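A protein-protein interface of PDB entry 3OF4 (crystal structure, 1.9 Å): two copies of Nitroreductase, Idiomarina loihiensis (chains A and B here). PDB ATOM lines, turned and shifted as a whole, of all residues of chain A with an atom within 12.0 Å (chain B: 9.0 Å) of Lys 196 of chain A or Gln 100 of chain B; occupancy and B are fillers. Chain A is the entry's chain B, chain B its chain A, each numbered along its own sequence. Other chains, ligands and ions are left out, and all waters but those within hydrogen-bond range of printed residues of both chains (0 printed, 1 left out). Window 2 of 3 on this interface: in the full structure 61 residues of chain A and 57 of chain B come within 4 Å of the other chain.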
ATOM      1  N   GLN A   8       6.953   4.429  17.215  1.00  0.00           N
ATOM      2  CA  GLN A   8       6.714   5.621  18.025  1.00  0.00           C
ATOM      3  C   GLN A   8       6.134   6.807  17.253  1.00  0.00           C
ATOM      4  O   GLN A   8       5.320   7.547  17.803  1.00  0.00           O
ATOM      5  CB  GLN A   8       8.010   6.066  18.699  1.00  0.00           C
ATOM      6  CG  GLN A   8       8.512   5.075  19.775  1.00  0.00           C
ATOM      7  CD  GLN A   8       7.858   5.301  21.093  1.00  0.00           C
ATOM      8  OE1 GLN A   8       6.632   5.492  21.176  1.00  0.00           O
ATOM      9  NE2 GLN A   8       8.665   5.267  22.160  1.00  0.00           N
ATOM     10  N   GLN A   9       6.563   6.987  16.003  1.00  0.00           N
ATOM     11  CA  GLN A   9       6.103   8.084  15.154  1.00  0.00           C
ATOM     12  C   GLN A   9       4.706   7.828  14.541  1.00  0.00           C
ATOM     13  O   GLN A   9       3.939   8.760  14.322  1.00  0.00           O
ATOM     14  CB  GLN A   9       7.135   8.355  14.044  1.00  0.00           C
ATOM     15  CG  GLN A   9       8.530   8.747  14.585  1.00  0.00           C
ATOM     16  CD  GLN A   9       8.564  10.146  15.229  1.00  0.00           C
ATOM     17  OE1 GLN A   9       7.540  10.847  15.319  1.00  0.00           O
ATOM     18  NE2 GLN A   9       9.761  10.569  15.646  1.00  0.00           N
ATOM     19  N   TRP A  10       4.375   6.559  14.308  1.00  0.00           N
ATOM     20  CA  TRP A  10       3.072   6.187  13.738  1.00  0.00           C
ATOM     21  C   TRP A  10       1.925   6.392  14.755  1.00  0.00           C
ATOM     22  O   TRP A  10       0.842   6.856  14.390  1.00  0.00           O
ATOM     23  CB  TRP A  10       3.105   4.732  13.275  1.00  0.00           C
ATOM     24  CG  TRP A  10       1.851   4.313  12.591  1.00  0.00           C
ATOM     25  CD1 TRP A  10       1.568   4.388  11.238  1.00  0.00           C
ATOM     26  CD2 TRP A  10       0.695   3.799  13.217  1.00  0.00           C
ATOM     27  NE1 TRP A  10       0.300   3.927  11.003  1.00  0.00           N
ATOM     28  CE2 TRP A  10      -0.272   3.589  12.200  1.00  0.00           C
ATOM     29  CE3 TRP A  10       0.361   3.515  14.545  1.00  0.00           C
ATOM     30  CZ2 TRP A  10      -1.521   3.073  12.471  1.00  0.00           C
ATOM     31  CZ3 TRP A  10      -0.863   3.013  14.812  1.00  0.00           C
ATOM     32  CH2 TRP A  10      -1.816   2.817  13.774  1.00  0.00           C
ATOM     33  N   ARG A  11       2.144   6.012  16.008  1.00  0.00           N
ATOM     34  CA  ARG A  11       1.054   6.020  16.989  1.00  0.00           C
ATOM     35  C   ARG A  11       0.787   7.434  17.420  1.00  0.00           C
ATOM     36  O   ARG A  11       1.628   8.330  17.230  1.00  0.00           O
ATOM     37  CB  ARG A  11       1.396   5.173  18.230  1.00  0.00           C
ATOM     38  CG  ARG A  11       2.634   5.678  19.007  1.00  0.00           C
ATOM     39  CD  ARG A  11       2.631   5.169  20.476  1.00  0.00           C
ATOM     40  NE  ARG A  11       1.424   5.642  21.142  1.00  0.00           N
ATOM     41  CZ  ARG A  11       1.235   6.902  21.534  1.00  0.00           C
ATOM     42  NH1 ARG A  11       2.186   7.801  21.401  1.00  0.00           N
ATOM     43  NH2 ARG A  11       0.100   7.271  22.088  1.00  0.00           N
ATOM     44  N   TYR A  12      -0.377   7.621  18.020  1.00  0.00           N
ATOM     45  CA  TYR A  12      -0.715   8.870  18.644  1.00  0.00           C
ATOM     46  C   TYR A  12      -1.923   8.619  19.572  1.00  0.00           C
ATOM     47  O   TYR A  12      -2.561   7.551  19.504  1.00  0.00           O
ATOM     48  CB  TYR A  12      -1.011   9.957  17.567  1.00  0.00           C
ATOM     49  CG  TYR A  12      -2.373   9.845  16.929  1.00  0.00           C
ATOM     50  CD1 TYR A  12      -2.675   8.794  16.080  1.00  0.00           C
ATOM     51  CD2 TYR A  12      -3.349  10.800  17.154  1.00  0.00           C
ATOM     52  CE1 TYR A  12      -3.915   8.675  15.490  1.00  0.00           C
ATOM     53  CE2 TYR A  12      -4.594  10.707  16.546  1.00  0.00           C
ATOM     54  CZ  TYR A  12      -4.877   9.625  15.733  1.00  0.00           C
ATOM     55  OH  TYR A  12      -6.110   9.502  15.157  1.00  0.00           O
ATOM     56  N   ALA A  13      -2.195   9.576  20.453  1.00  0.00           N
ATOM     57  CA  ALA A  13      -3.325   9.539  21.394  1.00  0.00           C
ATOM     58  C   ALA A  13      -4.610   9.839  20.613  1.00  0.00           C
ATOM     59  O   ALA A  13      -5.073  10.982  20.558  1.00  0.00           O
ATOM     60  CB  ALA A  13      -3.111  10.572  22.568  1.00  0.00           C
ATOM     61  N   ARG A 186      -8.297   4.808  13.673  1.00  0.00           N
ATOM     62  CA  ARG A 186      -8.589   6.244  13.730  1.00  0.00           C
ATOM     63  C   ARG A 186      -9.669   6.593  12.708  1.00  0.00           C
ATOM     64  O   ARG A 186      -9.744   5.982  11.635  1.00  0.00           O
ATOM     65  CB  ARG A 186      -7.328   7.072  13.439  1.00  0.00           C
ATOM     66  CG  ARG A 186      -6.804   6.847  12.005  1.00  0.00           C
ATOM     67  CD  ARG A 186      -5.437   7.400  11.816  1.00  0.00           C
ATOM     68  NE  ARG A 186      -4.445   6.632  12.529  1.00  0.00           N
ATOM     69  CZ  ARG A 186      -3.161   6.938  12.570  1.00  0.00           C
ATOM     70  NH1 ARG A 186      -2.687   8.005  11.936  1.00  0.00           N
ATOM     71  NH2 ARG A 186      -2.348   6.206  13.300  1.00  0.00           N
ATOM     72  N   ASP A 190     -10.288  12.517  12.143  1.00  0.00           N
ATOM     73  CA  ASP A 190      -9.525  12.885  13.320  1.00  0.00           C
ATOM     74  C   ASP A 190      -8.308  13.716  12.889  1.00  0.00           C
ATOM     75  O   ASP A 190      -7.231  13.191  12.577  1.00  0.00           O
ATOM     76  CB  ASP A 190      -9.061  11.659  14.122  1.00  0.00           C
ATOM     77  CG  ASP A 190      -8.345  12.038  15.422  1.00  0.00           C
ATOM     78  OD1 ASP A 190      -8.166  13.249  15.715  1.00  0.00           O
ATOM     79  OD2 ASP A 190      -7.927  11.114  16.155  1.00  0.00           O
ATOM     80  N   THR A 191      -8.477  15.020  12.936  1.00  0.00           N
ATOM     81  CA  THR A 191      -7.462  15.939  12.425  1.00  0.00           C
ATOM     82  C   THR A 191      -6.264  15.993  13.364  1.00  0.00           C
ATOM     83  O   THR A 191      -5.208  16.460  12.962  1.00  0.00           O
ATOM     84  CB  THR A 191      -8.025  17.360  12.269  1.00  0.00           C
ATOM     85  OG1 THR A 191      -8.422  17.836  13.564  1.00  0.00           O
ATOM     86  CG2 THR A 191      -9.207  17.395  11.297  1.00  0.00           C
ATOM     87  N   THR A 192      -6.411  15.496  14.604  1.00  0.00           N
ATOM     88  CA  THR A 192      -5.325  15.552  15.579  1.00  0.00           C
ATOM     89  C   THR A 192      -4.190  14.611  15.224  1.00  0.00           C
ATOM     90  O   THR A 192      -3.075  14.776  15.737  1.00  0.00           O
ATOM     91  CB  THR A 192      -5.777  15.220  17.032  1.00  0.00           C
ATOM     92  OG1 THR A 192      -6.102  13.828  17.123  1.00  0.00           O
ATOM     93  CG2 THR A 192      -7.002  16.125  17.432  1.00  0.00           C
ATOM     94  N   GLN A 193      -4.459  13.640  14.360  1.00  0.00           N
ATOM     95  CA  GLN A 193      -3.394  12.770  13.857  1.00  0.00           C
ATOM     96  C   GLN A 193      -2.367  13.564  13.037  1.00  0.00           C
ATOM     97  O   GLN A 193      -1.270  13.068  12.806  1.00  0.00           O
ATOM     98  CB  GLN A 193      -3.980  11.657  12.998  1.00  0.00           C
ATOM     99  CG  GLN A 193      -4.510  12.110  11.652  1.00  0.00           C
ATOM    100  CD  GLN A 193      -5.180  11.019  10.876  1.00  0.00           C
ATOM    101  OE1 GLN A 193      -4.509  10.200  10.269  1.00  0.00           O
ATOM    102  NE2 GLN A 193      -6.513  11.026  10.844  1.00  0.00           N
ATOM    103  N   PHE A 194      -2.725  14.756  12.548  1.00  0.00           N
ATOM    104  CA  PHE A 194      -1.775  15.576  11.771  1.00  0.00           C
ATOM    105  C   PHE A 194      -1.065  16.679  12.567  1.00  0.00           C
ATOM    106  O   PHE A 194      -0.371  17.499  12.004  1.00  0.00           O
ATOM    107  CB  PHE A 194      -2.446  16.130  10.502  1.00  0.00           C
ATOM    108  CG  PHE A 194      -3.095  15.059   9.675  1.00  0.00           C
ATOM    109  CD1 PHE A 194      -2.330  14.026   9.143  1.00  0.00           C
ATOM    110  CD2 PHE A 194      -4.471  15.023   9.502  1.00  0.00           C
ATOM    111  CE1 PHE A 194      -2.930  12.995   8.409  1.00  0.00           C
ATOM    112  CE2 PHE A 194      -5.069  14.005   8.746  1.00  0.00           C
ATOM    113  CZ  PHE A 194      -4.295  12.987   8.215  1.00  0.00           C
ATOM    114  N   GLN A 195      -1.230  16.685  13.879  1.00  0.00           N
ATOM    115  CA  GLN A 195      -0.428  17.532  14.763  1.00  0.00           C
ATOM    116  C   GLN A 195       1.005  17.009  14.896  1.00  0.00           C
ATOM    117  O   GLN A 195       1.194  15.826  15.080  1.00  0.00           O
ATOM    118  CB  GLN A 195      -1.055  17.541  16.150  1.00  0.00           C
ATOM    119  CG  GLN A 195      -2.433  18.153  16.153  1.00  0.00           C
ATOM    120  CD  GLN A 195      -2.854  18.585  17.524  1.00  0.00           C
ATOM    121  OE1 GLN A 195      -3.095  17.759  18.439  1.00  0.00           O
ATOM    122  NE2 GLN A 195      -2.932  19.882  17.692  1.00  0.00           N
ATOM    123  N   LYS A 196       2.005  17.890  14.853  1.00  0.00           N
ATOM    124  CA  LYS A 196       3.390  17.452  15.078  1.00  0.00           C
ATOM    125  C   LYS A 196       3.563  16.930  16.514  1.00  0.00           C
ATOM    126  O   LYS A 196       3.015  17.481  17.470  1.00  0.00           O
ATOM    127  CB  LYS A 196       4.390  18.571  14.800  1.00  0.00           C
ATOM    128  CG  LYS A 196       4.623  18.886  13.327  1.00  0.00           C
ATOM    129  CD  LYS A 196       5.500  20.114  13.153  1.00  0.00           C
ATOM    130  CE  LYS A 196       6.010  20.265  11.714  1.00  0.00           C
ATOM    131  NZ  LYS A 196       5.396  21.391  10.906  1.00  0.00           N
ATOM    132  N   LYS A 197       4.289  15.844  16.649  1.00  0.00           N
ATOM    133  CA  LYS A 197       4.583  15.284  17.969  1.00  0.00           C
ATOM    134  C   LYS A 197       5.492  16.158  18.775  1.00  0.00           C
ATOM    135  O   LYS A 197       6.409  16.811  18.226  1.00  0.00           O
ATOM    136  CB  LYS A 197       5.238  13.921  17.833  1.00  0.00           C
ATOM    137  CG  LYS A 197       4.267  12.852  17.914  1.00  0.00           C
ATOM    138  CD  LYS A 197       4.892  11.457  17.960  1.00  0.00           C
ATOM    139  CE  LYS A 197       3.834  10.450  17.587  1.00  0.00           C
ATOM    140  NZ  LYS A 197       2.466  10.959  17.930  1.00  0.00           N
ATOM    141  N   VAL A 198       5.201  16.246  20.067  1.00  0.00           N
ATOM    142  CA  VAL A 198       6.013  17.032  20.988  1.00  0.00           C
ATOM    143  C   VAL A 198       6.668  16.058  21.991  1.00  0.00           C
ATOM    144  O   VAL A 198       5.988  15.295  22.674  1.00  0.00           O
ATOM    145  CB  VAL A 198       5.152  18.090  21.698  1.00  0.00           C
ATOM    146  CG1 VAL A 198       5.985  18.923  22.657  1.00  0.00           C
ATOM    147  CG2 VAL A 198       4.464  18.973  20.648  1.00  0.00           C
ATOM    148  N   ARG A 199       7.993  16.043  21.999  1.00  0.00           N
ATOM    149  CA  ARG A 199       8.791  15.240  22.927  1.00  0.00           C
ATOM    150  C   ARG A 199      10.025  15.999  23.321  1.00  0.00           C
ATOM    151  O   ARG A 199      10.521  16.780  22.529  1.00  0.00           O
ATOM    152  CB  ARG A 199       9.253  13.931  22.252  1.00  0.00           C
ATOM    153  CG  ARG A 199       8.150  12.987  21.850  1.00  0.00           C
ATOM    154  CD  ARG A 199       7.387  12.430  23.024  1.00  0.00           C
ATOM    155  NE  ARG A 199       6.468  11.405  22.586  1.00  0.00           N
ATOM    156  CZ  ARG A 199       5.224  11.597  22.124  1.00  0.00           C
ATOM    157  NH1 ARG A 199       4.692  12.792  22.051  1.00  0.00           N
ATOM    158  NH2 ARG A 199       4.502  10.552  21.740  1.00  0.00           N
ATOM    159  N   GLN A 200      10.499  15.779  24.551  1.00  0.00           N
ATOM    160  CA  GLN A 200      11.778  16.302  25.085  1.00  0.00           C
ATOM    161  C   GLN A 200      12.871  16.005  24.070  1.00  0.00           C
ATOM    162  O   GLN A 200      12.963  14.853  23.680  1.00  0.00           O
ATOM    163  CB  GLN A 200      12.186  15.493  26.344  1.00  0.00           C
ATOM    164  CG  GLN A 200      11.404  15.662  27.626  1.00  0.00           C
ATOM    165  CD  GLN A 200      12.239  15.284  28.863  1.00  0.00           C
ATOM    166  OE1 GLN A 200      13.390  15.651  28.960  1.00  0.00           O
ATOM    167  NE2 GLN A 200      11.646  14.571  29.799  1.00  0.00           N
ATOM    168  N   PRO A 201      13.713  16.951  23.702  1.00  0.00           N
ATOM    169  CA  PRO A 201      14.832  16.512  22.857  1.00  0.00           C
ATOM    170  C   PRO A 201      15.818  15.664  23.649  1.00  0.00           C
ATOM    171  O   PRO A 201      15.853  15.728  24.887  1.00  0.00           O
ATOM    172  CB  PRO A 201      15.496  17.794  22.430  1.00  0.00           C
ATOM    173  CG  PRO A 201      14.874  18.906  23.305  1.00  0.00           C
ATOM    174  CD  PRO A 201      13.694  18.402  23.975  1.00  0.00           C
ATOM    175  N   LEU A 202      16.644  14.905  22.941  1.00  0.00           N
ATOM    176  CA  LEU A 202      17.608  14.054  23.620  1.00  0.00           C
ATOM    177  C   LEU A 202      18.573  14.868  24.496  1.00  0.00           C
ATOM    178  O   LEU A 202      18.974  14.394  25.547  1.00  0.00           O
ATOM    179  CB  LEU A 202      18.367  13.180  22.595  1.00  0.00           C
ATOM    180  CG  LEU A 202      19.203  12.015  23.141  1.00  0.00           C
ATOM    181  CD1 LEU A 202      18.312  10.984  23.777  1.00  0.00           C
ATOM    182  CD2 LEU A 202      20.048  11.425  21.978  1.00  0.00           C
ATOM    183  N   SER A 203      18.910  16.099  24.114  1.00  0.00           N
ATOM    184  CA  SER A 203      19.858  16.903  24.903  1.00  0.00           C
ATOM    185  C   SER A 203      19.297  17.235  26.288  1.00  0.00           C
ATOM    186  O   SER A 203      20.057  17.526  27.197  1.00  0.00           O
ATOM    187  CB  SER A 203      20.214  18.194  24.182  1.00  0.00           C
ATOM    188  OG  SER A 203      19.026  18.920  23.899  1.00  0.00           O
ATOM    189  N   ARG A 204      17.974  17.174  26.446  1.00  0.00           N
ATOM    190  CA  ARG A 204      17.364  17.419  27.753  1.00  0.00           C
ATOM    191  C   ARG A 204      17.025  16.093  28.434  1.00  0.00           C
ATOM    192  O   ARG A 204      17.220  15.965  29.628  1.00  0.00           O
ATOM    193  CB  ARG A 204      16.108  18.315  27.641  1.00  0.00           C
ATOM    194  CG  ARG A 204      16.357  19.761  27.223  1.00  0.00           C
ATOM    195  CD  ARG A 204      15.124  20.664  27.590  1.00  0.00           C
ATOM    196  N   ARG B  35      12.842   8.217  24.614  1.00  0.00           N
ATOM    197  CA  ARG B  35      12.343   9.604  24.715  1.00  0.00           C
ATOM    198  C   ARG B  35      11.027   9.906  23.969  1.00  0.00           C
ATOM    199  O   ARG B  35      10.358  10.895  24.261  1.00  0.00           O
ATOM    200  CB  ARG B  35      13.417  10.647  24.364  1.00  0.00           C
ATOM    201  CG  ARG B  35      13.405  11.092  22.981  1.00  0.00           C
ATOM    202  CD  ARG B  35      14.530  12.095  22.703  1.00  0.00           C
ATOM    203  NE  ARG B  35      14.556  12.177  21.281  1.00  0.00           N
ATOM    204  CZ  ARG B  35      13.755  12.928  20.558  1.00  0.00           C
ATOM    205  NH1 ARG B  35      12.919  13.816  21.114  1.00  0.00           N
ATOM    206  NH2 ARG B  35      13.852  12.825  19.270  1.00  0.00           N
ATOM    207  N   TYR B  93       8.244  21.589  28.532  1.00  0.00           N
ATOM    208  CA  TYR B  93       7.170  21.190  27.660  1.00  0.00           C
ATOM    209  C   TYR B  93       6.693  22.339  26.791  1.00  0.00           C
ATOM    210  O   TYR B  93       6.663  22.218  25.577  1.00  0.00           O
ATOM    211  CB  TYR B  93       5.970  20.590  28.425  1.00  0.00           C
ATOM    212  CG  TYR B  93       4.849  20.143  27.492  1.00  0.00           C
ATOM    213  CD1 TYR B  93       5.037  19.099  26.620  1.00  0.00           C
ATOM    214  CD2 TYR B  93       3.608  20.780  27.489  1.00  0.00           C
ATOM    215  CE1 TYR B  93       4.020  18.703  25.737  1.00  0.00           C
ATOM    216  CE2 TYR B  93       2.580  20.374  26.598  1.00  0.00           C
ATOM    217  CZ  TYR B  93       2.804  19.350  25.745  1.00  0.00           C
ATOM    218  OH  TYR B  93       1.833  18.936  24.871  1.00  0.00           O
ATOM    219  N   ILE B  94       6.337  23.465  27.401  1.00  0.00           N
ATOM    220  CA  ILE B  94       5.822  24.620  26.639  1.00  0.00           C
ATOM    221  C   ILE B  94       6.833  25.085  25.590  1.00  0.00           C
ATOM    222  O   ILE B  94       6.467  25.526  24.498  1.00  0.00           O
ATOM    223  CB  ILE B  94       5.441  25.804  27.565  1.00  0.00           C
ATOM    224  CG1 ILE B  94       4.323  25.401  28.537  1.00  0.00           C
ATOM    225  CG2 ILE B  94       5.024  27.058  26.733  1.00  0.00           C
ATOM    226  CD1 ILE B  94       2.994  24.969  27.929  1.00  0.00           C
ATOM    227  N   SER B  95       8.115  25.031  25.933  1.00  0.00           N
ATOM    228  CA  SER B  95       9.154  25.461  25.008  1.00  0.00           C
ATOM    229  C   SER B  95       9.136  24.592  23.740  1.00  0.00           C
ATOM    230  O   SER B  95       9.138  25.107  22.628  1.00  0.00           O
ATOM    231  CB  SER B  95      10.514  25.397  25.695  1.00  0.00           C
ATOM    232  OG  SER B  95      11.534  25.813  24.826  1.00  0.00           O
ATOM    233  N   GLU B  96       9.104  23.287  23.924  1.00  0.00           N
ATOM    234  CA  GLU B  96       9.043  22.365  22.774  1.00  0.00           C
ATOM    235  C   GLU B  96       7.680  22.436  22.036  1.00  0.00           C
ATOM    236  O   GLU B  96       7.635  22.458  20.803  1.00  0.00           O
ATOM    237  CB  GLU B  96       9.342  20.955  23.244  1.00  0.00           C
ATOM    238  CG  GLU B  96       9.538  19.938  22.128  1.00  0.00           C
ATOM    239  CD  GLU B  96      10.820  20.137  21.308  1.00  0.00           C
ATOM    240  OE1 GLU B  96      11.749  20.845  21.768  1.00  0.00           O
ATOM    241  OE2 GLU B  96      10.896  19.566  20.200  1.00  0.00           O
ATOM    242  N   LEU B  97       6.583  22.513  22.786  1.00  0.00           N
ATOM    243  CA  LEU B  97       5.255  22.658  22.189  1.00  0.00           C
ATOM    244  C   LEU B  97       5.153  23.892  21.307  1.00  0.00           C
ATOM    245  O   LEU B  97       4.628  23.852  20.200  1.00  0.00           O
ATOM    246  CB  LEU B  97       4.211  22.787  23.293  1.00  0.00           C
ATOM    247  CG  LEU B  97       2.757  23.022  22.913  1.00  0.00           C
ATOM    248  CD1 LEU B  97       2.245  21.860  22.104  1.00  0.00           C
ATOM    249  CD2 LEU B  97       1.928  23.252  24.184  1.00  0.00           C
ATOM    250  N   SER B  98       5.657  25.011  21.822  1.00  0.00           N
ATOM    251  CA  SER B  98       5.583  26.278  21.135  1.00  0.00           C
ATOM    252  C   SER B  98       6.357  26.235  19.829  1.00  0.00           C
ATOM    253  O   SER B  98       5.905  26.746  18.811  1.00  0.00           O
ATOM    254  CB  SER B  98       6.153  27.391  22.020  1.00  0.00           C
ATOM    255  OG  SER B  98       6.258  28.589  21.281  1.00  0.00           O
ATOM    256  N   GLN B  99       7.539  25.638  19.881  1.00  0.00           N
ATOM    257  CA  GLN B  99       8.411  25.536  18.712  1.00  0.00           C
ATOM    258  C   GLN B  99       7.822  24.614  17.636  1.00  0.00           C
ATOM    259  O   GLN B  99       7.859  24.948  16.454  1.00  0.00           O
ATOM    260  CB  GLN B  99       9.801  25.016  19.122  1.00  0.00           C
ATOM    261  CG  GLN B  99      10.752  24.657  17.950  1.00  0.00           C
ATOM    262  N   GLN B 100       7.308  23.462  18.050  1.00  0.00           N
ATOM    263  CA  GLN B 100       6.834  22.429  17.094  1.00  0.00           C
ATOM    264  C   GLN B 100       5.488  22.776  16.452  1.00  0.00           C
ATOM    265  O   GLN B 100       5.282  22.535  15.265  1.00  0.00           O
ATOM    266  CB  GLN B 100       6.726  21.066  17.769  1.00  0.00           C
ATOM    267  CG  GLN B 100       8.071  20.389  18.069  1.00  0.00           C
ATOM    268  CD  GLN B 100       8.923  20.226  16.837  1.00  0.00           C
ATOM    269  OE1 GLN B 100       8.484  19.679  15.841  1.00  0.00           O
ATOM    270  NE2 GLN B 100      10.147  20.718  16.904  1.00  0.00           N
ATOM    271  N   ARG B 101       4.585  23.350  17.238  1.00  0.00           N
ATOM    272  CA  ARG B 101       3.243  23.679  16.768  1.00  0.00           C
ATOM    273  C   ARG B 101       3.043  25.146  16.515  1.00  0.00           C
ATOM    274  O   ARG B 101       1.920  25.570  16.227  1.00  0.00           O
ATOM    275  CB  ARG B 101       2.238  23.156  17.765  1.00  0.00           C
ATOM    276  CG  ARG B 101       2.323  21.689  17.829  1.00  0.00           C
ATOM    277  CD  ARG B 101       1.114  21.087  18.378  1.00  0.00           C
ATOM    278  NE  ARG B 101       1.333  19.664  18.524  1.00  0.00           N
ATOM    279  CZ  ARG B 101       0.656  18.920  19.383  1.00  0.00           C
ATOM    280  NH1 ARG B 101      -0.280  19.488  20.117  1.00  0.00           N
ATOM    281  NH2 ARG B 101       0.897  17.620  19.498  1.00  0.00           N
ATOM    282  N   GLN B 102       4.128  25.921  16.571  1.00  0.00           N
ATOM    283  CA  GLN B 102       4.079  27.329  16.246  1.00  0.00           C
ATOM    284  C   GLN B 102       2.992  28.123  16.988  1.00  0.00           C
ATOM    285  O   GLN B 102       2.230  28.866  16.376  1.00  0.00           O
ATOM    286  CB  GLN B 102       3.927  27.454  14.720  1.00  0.00           C
ATOM    287  CG  GLN B 102       5.130  26.833  13.989  1.00  0.00           C
ATOM    288  CD  GLN B 102       6.409  27.597  14.322  1.00  0.00           C
ATOM    289  OE1 GLN B 102       6.448  28.817  14.255  1.00  0.00           O
ATOM    290  NE2 GLN B 102       7.428  26.882  14.736  1.00  0.00           N
ATOM    291  N   LEU B 103       2.929  27.996  18.301  1.00  0.00           N
ATOM    292  CA  LEU B 103       1.906  28.720  19.063  1.00  0.00           C
ATOM    293  C   LEU B 103       2.227  30.203  19.153  1.00  0.00           C
ATOM    294  O   LEU B 103       3.388  30.604  19.113  1.00  0.00           O
ATOM    295  CB  LEU B 103       1.749  28.144  20.478  1.00  0.00           C
ATOM    296  CG  LEU B 103       1.448  26.665  20.677  1.00  0.00           C
ATOM    297  CD1 LEU B 103       1.075  26.431  22.148  1.00  0.00           C
ATOM    298  CD2 LEU B 103       0.357  26.143  19.738  1.00  0.00           C
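The guanidinium group (NH1) of Arg 35 of chain B is in hydrogen-bond range of the backbone carbonyl oxygen (O) of Gln 200 of chain A. O of Lys 196 of chain A sits at hydrogen-bond distance from NH2 of Arg 101 of chain B (2.9 Å).
No position is printed for both chains.
Of the 22 printed residues of chain A, 8 touch a printed residue of chain B. Hydrophobic or aromatic side chains of chain A that line the printed part of chain B: Val 198, Pro 201 and Leu 202. Along chain A the printed residues that touch a printed residue of chain B span positions 195 to 202.
Printed residues of chain B within 4 Å of Lys 196 of chain A: Gln 100 (3.2 Å) and Arg 101 (2.9 Å). Of the printed residues of chain B, Gln 200 of chain A touches Arg 35. Of the printed residues of chain B, Leu 202 of chain A touches Arg 35 (3.5 Å). Printed residues of chain A within 4 Å of Tyr 93 of chain B: Val 198 (3.7 Å). Of the printed residues of chain A, Leu 97 of chain B touches Val 198. No residue of chain A comes within 4 Å of Gln 99 of chain B. Gln 100 of chain B touches just these residues of chain A: Lys 196 (3.2 Å) and Lys 197 (3.9 Å). No residue of chain A comes within 4 Å of Gln 102 of chain B. The nearest residue of chain B that does not touch Lys 196 of chain A is Gln 102 of chain B (6.3 Å).
The side-chain amino group (NZ) of Lys 197 of chain A lies within hydrogen-bond range of the backbone carbonyl oxygen (O) of Arg 11 of chain A, at 2.8 Å.
Among the printed residues, merely in contact across the chains: Lys 196 of chain A with Gln 100 of chain B, Arg 199 of chain A with Glu 96 of chain B, Leu 202 of chain A with Arg 35 of chain B, Arg 199 of chain A with Arg 35 of chain B, Gln 195 of chain A with Arg 101 of chain B, Val 198 of chain A with Leu 97 of chain B, Val 198 of chain A with Tyr 93 of chain B, Val 198 of chain A with Glu 96 of chain B, Pro 201 of chain A with Arg 35 of chain B, Pro 201 of chain A with Glu 96 of chain B, Val 198 of chain A with Arg 101 of chain B and Lys 197 of chain A with Gln 100 of chain B.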
